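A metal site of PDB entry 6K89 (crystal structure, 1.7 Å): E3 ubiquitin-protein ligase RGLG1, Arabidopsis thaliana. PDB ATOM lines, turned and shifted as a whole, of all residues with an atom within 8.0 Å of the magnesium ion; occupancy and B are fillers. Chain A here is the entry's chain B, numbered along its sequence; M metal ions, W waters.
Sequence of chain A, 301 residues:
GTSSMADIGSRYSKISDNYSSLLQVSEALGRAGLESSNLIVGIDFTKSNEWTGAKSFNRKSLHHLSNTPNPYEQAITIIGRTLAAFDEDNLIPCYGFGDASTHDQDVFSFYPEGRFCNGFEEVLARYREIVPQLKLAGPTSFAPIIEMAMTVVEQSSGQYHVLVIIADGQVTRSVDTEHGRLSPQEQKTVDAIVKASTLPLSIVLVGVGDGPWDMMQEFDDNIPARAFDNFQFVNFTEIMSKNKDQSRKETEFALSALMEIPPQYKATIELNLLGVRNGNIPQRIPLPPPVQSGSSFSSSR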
ATOM      1  N   ASP A  44     -13.627  -7.072  24.239  1.00  0.00           N
ATOM      2  CA  ASP A  44     -13.088  -8.172  25.037  1.00  0.00           C
ATOM      3  C   ASP A  44     -11.579  -8.226  24.906  1.00  0.00           C
ATOM      4  O   ASP A  44     -11.047  -8.428  23.804  1.00  0.00           O
ATOM      5  CB  ASP A  44     -13.739  -9.477  24.554  1.00  0.00           C
ATOM      6  CG  ASP A  44     -13.295 -10.713  25.328  1.00  0.00           C
ATOM      7  OD1 ASP A  44     -12.093 -10.939  25.583  1.00  0.00           O
ATOM      8  OD2 ASP A  44     -14.204 -11.492  25.677  1.00  0.00           O
ATOM      9  N   PHE A  45     -10.880  -8.052  26.028  1.00  0.00           N
ATOM     10  CA  PHE A  45      -9.427  -8.140  26.056  1.00  0.00           C
ATOM     11  C   PHE A  45      -8.954  -9.284  26.954  1.00  0.00           C
ATOM     12  O   PHE A  45      -7.944  -9.149  27.672  1.00  0.00           O
ATOM     13  CB  PHE A  45      -8.832  -6.804  26.518  1.00  0.00           C
ATOM     14  CG  PHE A  45      -8.954  -5.697  25.508  1.00  0.00           C
ATOM     15  CD1 PHE A  45      -8.342  -5.788  24.268  1.00  0.00           C
ATOM     16  CD2 PHE A  45      -9.671  -4.548  25.799  1.00  0.00           C
ATOM     17  CE1 PHE A  45      -8.454  -4.777  23.336  1.00  0.00           C
ATOM     18  CE2 PHE A  45      -9.773  -3.517  24.869  1.00  0.00           C
ATOM     19  CZ  PHE A  45      -9.166  -3.635  23.632  1.00  0.00           C
ATOM     20  N   THR A  46      -9.688 -10.400  26.939  1.00  0.00           N
ATOM     21  CA  THR A  46      -9.305 -11.565  27.727  1.00  0.00           C
ATOM     22  C   THR A  46      -8.174 -12.346  27.048  1.00  0.00           C
ATOM     23  O   THR A  46      -7.966 -12.246  25.833  1.00  0.00           O
ATOM     24  CB  THR A  46     -10.500 -12.531  27.988  1.00  0.00           C
ATOM     25  OG1 THR A  46     -11.076 -12.939  26.753  1.00  0.00           O
ATOM     26  CG2 THR A  46     -11.561 -11.849  28.845  1.00  0.00           C
ATOM     27  N   LYS A  47      -7.459 -13.146  27.837  1.00  0.00           N
ATOM     28  CA  LYS A  47      -6.275 -13.833  27.359  1.00  0.00           C
ATOM     29  C   LYS A  47      -6.596 -14.918  26.347  1.00  0.00           C
ATOM     30  O   LYS A  47      -5.766 -15.233  25.492  1.00  0.00           O
ATOM     31  CB  LYS A  47      -5.480 -14.423  28.525  1.00  0.00           C
ATOM     32  CG  LYS A  47      -4.043 -14.781  28.128  1.00  0.00           C
ATOM     33  CD  LYS A  47      -3.047 -14.504  29.234  1.00  0.00           C
ATOM     34  CE  LYS A  47      -1.631 -14.715  28.744  1.00  0.00           C
ATOM     35  NZ  LYS A  47      -1.472 -16.093  28.214  1.00  0.00           N
ATOM     36  N   SER A  48      -7.806 -15.480  26.405  1.00  0.00           N
ATOM     37  CA  SER A  48      -8.191 -16.506  25.440  1.00  0.00           C
ATOM     38  C   SER A  48      -8.079 -16.018  23.987  1.00  0.00           C
ATOM     39  O   SER A  48      -7.964 -16.828  23.076  1.00  0.00           O
ATOM     40  CB  SER A  48      -9.599 -17.014  25.707  1.00  0.00           C
ATOM     41  OG  SER A  48     -10.570 -16.044  25.360  1.00  0.00           O
ATOM     42  N   ASN A  49      -8.097 -14.699  23.772  1.00  0.00           N
ATOM     43  CA  ASN A  49      -7.872 -14.166  22.424  1.00  0.00           C
ATOM     44  C   ASN A  49      -6.554 -14.643  21.807  1.00  0.00           C
ATOM     45  O   ASN A  49      -6.394 -14.600  20.590  1.00  0.00           O
ATOM     46  CB  ASN A  49      -7.880 -12.642  22.428  1.00  0.00           C
ATOM     47  CG  ASN A  49      -9.276 -12.058  22.500  1.00  0.00           C
ATOM     48  OD1 ASN A  49     -10.021 -12.076  21.521  1.00  0.00           O
ATOM     49  ND2 ASN A  49      -9.624 -11.502  23.667  1.00  0.00           N
ATOM     50  N   GLU A  50      -5.636 -15.079  22.657  1.00  0.00           N
ATOM     51  CA  GLU A  50      -4.354 -15.590  22.176  1.00  0.00           C
ATOM     52  C   GLU A  50      -4.505 -16.927  21.449  1.00  0.00           C
ATOM     53  O   GLU A  50      -3.711 -17.246  20.555  1.00  0.00           O
ATOM     54  CB  GLU A  50      -3.366 -15.709  23.345  1.00  0.00           C
ATOM     55  CG  GLU A  50      -2.860 -14.349  23.815  1.00  0.00           C
ATOM     56  CD  GLU A  50      -1.841 -14.421  24.936  1.00  0.00           C
ATOM     57  OE1 GLU A  50      -1.441 -13.350  25.425  1.00  0.00           O
ATOM     58  OE2 GLU A  50      -1.442 -15.534  25.339  1.00  0.00           O
ATOM     59  N   TRP A  51      -5.521 -17.709  21.801  1.00  0.00           N
ATOM     60  CA  TRP A  51      -5.605 -19.040  21.209  1.00  0.00           C
ATOM     61  C   TRP A  51      -6.906 -19.350  20.432  1.00  0.00           C
ATOM     62  O   TRP A  51      -6.994 -20.351  19.736  1.00  0.00           O
ATOM     63  CB  TRP A  51      -5.384 -20.087  22.292  1.00  0.00           C
ATOM     64  CG  TRP A  51      -6.382 -20.130  23.419  1.00  0.00           C
ATOM     65  CD1 TRP A  51      -7.618 -20.707  23.400  1.00  0.00           C
ATOM     66  CD2 TRP A  51      -6.196 -19.629  24.748  1.00  0.00           C
ATOM     67  NE1 TRP A  51      -8.220 -20.591  24.628  1.00  0.00           N
ATOM     68  CE2 TRP A  51      -7.364 -19.927  25.472  1.00  0.00           C
ATOM     69  CE3 TRP A  51      -5.157 -18.951  25.387  1.00  0.00           C
ATOM     70  CZ2 TRP A  51      -7.531 -19.570  26.809  1.00  0.00           C
ATOM     71  CZ3 TRP A  51      -5.315 -18.603  26.718  1.00  0.00           C
ATOM     72  CH2 TRP A  51      -6.499 -18.901  27.412  1.00  0.00           C
ATOM     73  N   THR A  52      -7.897 -18.470  20.532  1.00  0.00           N
ATOM     74  CA  THR A  52      -9.165 -18.723  19.830  1.00  0.00           C
ATOM     75  C   THR A  52      -9.083 -18.363  18.338  1.00  0.00           C
ATOM     76  O   THR A  52     -10.062 -18.512  17.604  1.00  0.00           O
ATOM     77  CB  THR A  52     -10.315 -17.955  20.480  1.00  0.00           C
ATOM     78  OG1 THR A  52      -9.964 -16.569  20.574  1.00  0.00           O
ATOM     79  CG2 THR A  52     -10.589 -18.498  21.873  1.00  0.00           C
ATOM     80  N   LEU A  62      -6.254 -12.893  18.239  1.00  0.00           N
ATOM     81  CA  LEU A  62      -7.342 -12.149  17.612  1.00  0.00           C
ATOM     82  C   LEU A  62      -7.112 -10.638  17.725  1.00  0.00           C
ATOM     83  O   LEU A  62      -7.719  -9.845  16.991  1.00  0.00           O
ATOM     84  CB  LEU A  62      -8.688 -12.530  18.239  1.00  0.00           C
ATOM     85  CG  LEU A  62      -9.173 -13.954  18.005  1.00  0.00           C
ATOM     86  CD1 LEU A  62     -10.587 -14.122  18.527  1.00  0.00           C
ATOM     87  CD2 LEU A  62      -9.124 -14.300  16.529  1.00  0.00           C
ATOM     88  N   TYR A  72     -11.679  -8.064  15.351  1.00  0.00           N
ATOM     89  CA  TYR A  72     -12.246  -6.955  16.097  1.00  0.00           C
ATOM     90  C   TYR A  72     -12.368  -5.722  15.213  1.00  0.00           C
ATOM     91  O   TYR A  72     -13.418  -5.090  15.144  1.00  0.00           O
ATOM     92  CB  TYR A  72     -11.415  -6.656  17.354  1.00  0.00           C
ATOM     93  CG  TYR A  72     -11.605  -7.702  18.424  1.00  0.00           C
ATOM     94  CD1 TYR A  72     -12.648  -7.610  19.335  1.00  0.00           C
ATOM     95  CD2 TYR A  72     -10.752  -8.794  18.518  1.00  0.00           C
ATOM     96  CE1 TYR A  72     -12.839  -8.563  20.309  1.00  0.00           C
ATOM     97  CE2 TYR A  72     -10.941  -9.767  19.497  1.00  0.00           C
ATOM     98  CZ  TYR A  72     -11.987  -9.648  20.391  1.00  0.00           C
ATOM     99  OH  TYR A  72     -12.179 -10.594  21.352  1.00  0.00           O
ATOM    100  N   PHE A  97     -12.741  -4.477  28.382  1.00  0.00           N
ATOM    101  CA  PHE A  97     -12.913  -5.276  29.589  1.00  0.00           C
ATOM    102  C   PHE A  97     -12.159  -6.580  29.433  1.00  0.00           C
ATOM    103  O   PHE A  97     -11.929  -7.045  28.316  1.00  0.00           O
ATOM    104  CB  PHE A  97     -14.398  -5.546  29.867  1.00  0.00           C
ATOM    105  CG  PHE A  97     -15.097  -6.330  28.783  1.00  0.00           C
ATOM    106  CD1 PHE A  97     -15.725  -5.677  27.712  1.00  0.00           C
ATOM    107  CD2 PHE A  97     -15.139  -7.711  28.819  1.00  0.00           C
ATOM    108  CE1 PHE A  97     -16.371  -6.399  26.711  1.00  0.00           C
ATOM    109  CE2 PHE A  97     -15.776  -8.442  27.814  1.00  0.00           C
ATOM    110  CZ  PHE A  97     -16.390  -7.797  26.762  1.00  0.00           C
ATOM    111  N   GLY A  98     -11.773  -7.177  30.566  1.00  0.00           N
ATOM    112  CA  GLY A  98     -11.184  -8.504  30.547  1.00  0.00           C
ATOM    113  C   GLY A  98      -9.666  -8.481  30.588  1.00  0.00           C
ATOM    114  O   GLY A  98      -9.041  -9.534  30.743  1.00  0.00           O
ATOM    115  N   ALA A 137      -6.355 -10.700  30.294  1.00  0.00           N
ATOM    116  CA  ALA A 137      -6.629 -11.468  31.490  1.00  0.00           C
ATOM    117  C   ALA A 137      -7.978 -12.195  31.417  1.00  0.00           C
ATOM    118  O   ALA A 137      -8.258 -12.929  30.466  1.00  0.00           O
ATOM    119  CB  ALA A 137      -6.551 -10.589  32.711  1.00  0.00           C
ATOM    120  N   GLY A 138      -8.791 -12.013  32.450  1.00  0.00           N
ATOM    121  CA  GLY A 138     -10.074 -12.695  32.538  1.00  0.00           C
ATOM    122  C   GLY A 138     -10.589 -12.571  33.956  1.00  0.00           C
ATOM    123  O   GLY A 138     -10.058 -11.790  34.731  1.00  0.00           O
ATOM    124  N   PRO A 139     -11.635 -13.342  34.291  1.00  0.00           N
ATOM    125  CA  PRO A 139     -12.382 -14.238  33.406  1.00  0.00           C
ATOM    126  C   PRO A 139     -13.390 -13.420  32.614  1.00  0.00           C
ATOM    127  O   PRO A 139     -13.272 -12.201  32.621  1.00  0.00           O
ATOM    128  CB  PRO A 139     -13.071 -15.180  34.367  1.00  0.00           C
ATOM    129  CG  PRO A 139     -13.331 -14.326  35.582  1.00  0.00           C
ATOM    130  CD  PRO A 139     -12.166 -13.362  35.670  1.00  0.00           C
ATOM    131  N   THR A 140     -14.376 -14.056  31.995  1.00  0.00           N
ATOM    132  CA  THR A 140     -15.311 -13.359  31.124  1.00  0.00           C
ATOM    133  C   THR A 140     -16.681 -13.108  31.766  1.00  0.00           C
ATOM    134  O   THR A 140     -17.401 -14.035  32.143  1.00  0.00           O
ATOM    135  CB  THR A 140     -15.507 -14.138  29.816  1.00  0.00           C
ATOM    136  OG1 THR A 140     -14.230 -14.335  29.198  1.00  0.00           O
ATOM    137  CG2 THR A 140     -16.433 -13.370  28.870  1.00  0.00           C
ATOM    138  N   PHE A 142     -20.046 -10.182  30.982  1.00  0.00           N
ATOM    139  CA  PHE A 142     -20.517  -9.011  30.239  1.00  0.00           C
ATOM    140  C   PHE A 142     -21.336  -8.076  31.116  1.00  0.00           C
ATOM    141  O   PHE A 142     -21.912  -7.088  30.635  1.00  0.00           O
ATOM    142  CB  PHE A 142     -21.328  -9.447  29.016  1.00  0.00           C
ATOM    143  CG  PHE A 142     -20.560 -10.362  28.088  1.00  0.00           C
ATOM    144  CD1 PHE A 142     -19.245 -10.067  27.743  1.00  0.00           C
ATOM    145  CD2 PHE A 142     -21.129 -11.524  27.609  1.00  0.00           C
ATOM    146  CE1 PHE A 142     -18.515 -10.911  26.908  1.00  0.00           C
ATOM    147  CE2 PHE A 142     -20.406 -12.380  26.783  1.00  0.00           C
ATOM    148  CZ  PHE A 142     -19.106 -12.061  26.427  1.00  0.00           C
ATOM    149  N   ALA A 167     -16.623 -10.135  21.407  1.00  0.00           N
ATOM    150  CA  ALA A 167     -15.950 -11.023  22.360  1.00  0.00           C
ATOM    151  C   ALA A 167     -15.535 -12.322  21.684  1.00  0.00           C
ATOM    152  O   ALA A 167     -16.094 -12.659  20.649  1.00  0.00           O
ATOM    153  CB  ALA A 167     -16.840 -11.325  23.551  1.00  0.00           C
ATOM    154  N   ASP A 168     -14.593 -13.042  22.290  1.00  0.00           N
ATOM    155  CA  ASP A 168     -14.127 -14.299  21.711  1.00  0.00           C
ATOM    156  C   ASP A 168     -14.489 -15.503  22.575  1.00  0.00           C
ATOM    157  O   ASP A 168     -13.991 -16.620  22.372  1.00  0.00           O
ATOM    158  CB  ASP A 168     -12.602 -14.269  21.494  1.00  0.00           C
ATOM    159  CG  ASP A 168     -11.833 -14.572  22.756  1.00  0.00           C
ATOM    160  OD1 ASP A 168     -12.228 -14.066  23.829  1.00  0.00           O
ATOM    161  OD2 ASP A 168     -10.847 -15.342  22.680  1.00  0.00           O
ATOM    162  N   GLY A 169     -15.372 -15.306  23.548  1.00  0.00           N
ATOM    163  CA  GLY A 169     -15.784 -16.426  24.361  1.00  0.00           C
ATOM    164  C   GLY A 169     -16.999 -16.086  25.189  1.00  0.00           C
ATOM    165  O   GLY A 169     -17.180 -14.926  25.566  1.00  0.00           O
ATOM    166  N   GLN A 170     -17.835 -17.096  25.444  1.00  0.00           N
ATOM    167  CA  GLN A 170     -19.012 -16.900  26.271  1.00  0.00           C
ATOM    168  C   GLN A 170     -18.599 -16.597  27.714  1.00  0.00           C
ATOM    169  O   GLN A 170     -17.470 -16.884  28.123  1.00  0.00           O
ATOM    170  CB  GLN A 170     -19.929 -18.131  26.207  1.00  0.00           C
ATOM    171  CG  GLN A 170     -21.105 -18.180  27.212  1.00  0.00           C
ATOM    172  CD  GLN A 170     -22.134 -17.049  27.034  1.00  0.00           C
ATOM    173  OE1 GLN A 170     -21.807 -15.920  26.663  1.00  0.00           O
ATOM    174  NE2 GLN A 170     -23.391 -17.367  27.310  1.00  0.00           N
ATOM    175  N   VAL A 171     -19.518 -15.994  28.462  1.00  0.00           N
ATOM    176  CA  VAL A 171     -19.391 -15.812  29.897  1.00  0.00           C
ATOM    177  C   VAL A 171     -18.864 -17.077  30.582  1.00  0.00           C
ATOM    178  O   VAL A 171     -19.295 -18.180  30.253  1.00  0.00           O
ATOM    179  CB  VAL A 171     -20.742 -15.437  30.503  1.00  0.00           C
ATOM    180  CG1 VAL A 171     -20.590 -15.156  31.978  1.00  0.00           C
ATOM    181  CG2 VAL A 171     -21.302 -14.210  29.808  1.00  0.00           C
ATOM    182  N   THR A 172     -17.945 -16.893  31.518  1.00  0.00           N
ATOM    183  CA  THR A 172     -17.316 -18.016  32.230  1.00  0.00           C
ATOM    184  C   THR A 172     -18.362 -18.832  32.969  1.00  0.00           C
ATOM    185  O   THR A 172     -19.225 -18.281  33.642  1.00  0.00           O
ATOM    186  CB  THR A 172     -16.241 -17.476  33.193  1.00  0.00           C
ATOM    187  OG1 THR A 172     -15.225 -16.823  32.423  1.00  0.00           O
ATOM    188  CG2 THR A 172     -15.618 -18.627  33.987  1.00  0.00           C
ATOM    189  N   VAL A 208     -16.424 -13.435  17.847  1.00  0.00           N
ATOM    190  CA  VAL A 208     -15.315 -13.598  16.914  1.00  0.00           C
ATOM    191  C   VAL A 208     -14.483 -14.801  17.356  1.00  0.00           C
ATOM    192  O   VAL A 208     -14.631 -15.295  18.476  1.00  0.00           O
ATOM    193  CB  VAL A 208     -14.407 -12.336  16.820  1.00  0.00           C
ATOM    194  CG1 VAL A 208     -15.139 -11.187  16.109  1.00  0.00           C
ATOM    195  CG2 VAL A 208     -13.947 -11.872  18.214  1.00  0.00           C
ATOM    196  N   GLY A 211     -14.513 -19.849  18.949  1.00  0.00           N
ATOM    197  CA  GLY A 211     -15.517 -20.214  19.925  1.00  0.00           C
ATOM    198  C   GLY A 211     -14.921 -21.060  21.036  1.00  0.00           C
ATOM    199  O   GLY A 211     -13.797 -20.810  21.475  1.00  0.00           O
ATOM    200  N   TRP A 213     -19.046 -21.511  20.288  1.00  0.00           N
ATOM    201  CA  TRP A 213     -20.227 -20.667  20.401  1.00  0.00           C
ATOM    202  C   TRP A 213     -21.525 -21.481  20.346  1.00  0.00           C
ATOM    203  O   TRP A 213     -22.603 -20.943  20.122  1.00  0.00           O
ATOM    204  CB  TRP A 213     -20.234 -19.610  19.298  1.00  0.00           C
ATOM    205  CG  TRP A 213     -19.170 -18.559  19.433  1.00  0.00           C
ATOM    206  CD1 TRP A 213     -18.101 -18.354  18.596  1.00  0.00           C
ATOM    207  CD2 TRP A 213     -19.071 -17.555  20.462  1.00  0.00           C
ATOM    208  NE1 TRP A 213     -17.342 -17.300  19.053  1.00  0.00           N
ATOM    209  CE2 TRP A 213     -17.910 -16.793  20.197  1.00  0.00           C
ATOM    210  CE3 TRP A 213     -19.834 -17.244  21.588  1.00  0.00           C
ATOM    211  CZ2 TRP A 213     -17.510 -15.732  21.005  1.00  0.00           C
ATOM    212  CZ3 TRP A 213     -19.439 -16.176  22.392  1.00  0.00           C
ATOM    213  CH2 TRP A 213     -18.295 -15.442  22.090  1.00  0.00           C
HETATM  214 MG    MG M   1     -12.202 -14.802  25.982  1.00  0.00          MG
HETATM  215  O   HOH W   1     -14.216 -13.799  26.454  1.00  0.00           O
HETATM  216  O   HOH W   2     -12.761 -16.888  27.082  1.00  0.00           O
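OG1 of Thr 52 is in hydrogen-bond range of OD2 of Asp 168, at 2.6 Å.
The side-chain carboxylate of Asp 168 lies within hydrogen-bond range of the backbone NH of Asn 49 (3.0 Å).
The side-chain amide nitrogen (ND2) of Asn 49 lies within hydrogen-bond range of the side-chain carboxylate (OD1) of Asp 44, 3.2 Å away.
The backbone carbonyl oxygen of Thr 46 is in hydrogen-bond range of the side-chain amide nitrogen of Asn 49.
N of Thr 140 is in hydrogen-bond range of OG1 of Thr 172 (2.9 Å).
The backbone carbonyl oxygen of Asp 44 is in hydrogen-bond range of the side-chain hydroxyl of Tyr 72 (3.5 Å).
The backbone carbonyl oxygen of Ser 48 sits at hydrogen-bond distance from the side-chain hydroxyl of Thr 52, at 3.2 Å.
N of Thr 46 is in hydrogen-bond range of OD1 of Asp 44 (2.8 Å).
Asp 44 touches the magnesium ion (OD2 to MG, 3.9 Å).
Thr 140 touches the magnesium ion.
Five residues have an atom within 4 Å of the magnesium ion: Asp 44, Thr 46, Ser 48, Thr 140 and Asp 168.
The nearest printed residue that does not touch the magnesium ion is Gly 169 (4.03 Å).
OG of Ser 48 is bound to the magnesium ion.
OD1 of Asp 168 is bound to the magnesium ion (2.3 Å).
Water W1 binds the magnesium ion.
OG1 of Thr 46 binds the magnesium ion (2.3 Å).
Water W2 binds the magnesium ion (2.4 Å).
Water W1 lies within hydrogen-bond range of the side-chain carboxylate (OD2) of Asp 44 (2.4 Å), the side-chain hydroxyl (OG1) of Thr 140 (2.8 Å) and the backbone carbonyl oxygen (O) of Gly 169 (3.3 Å).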
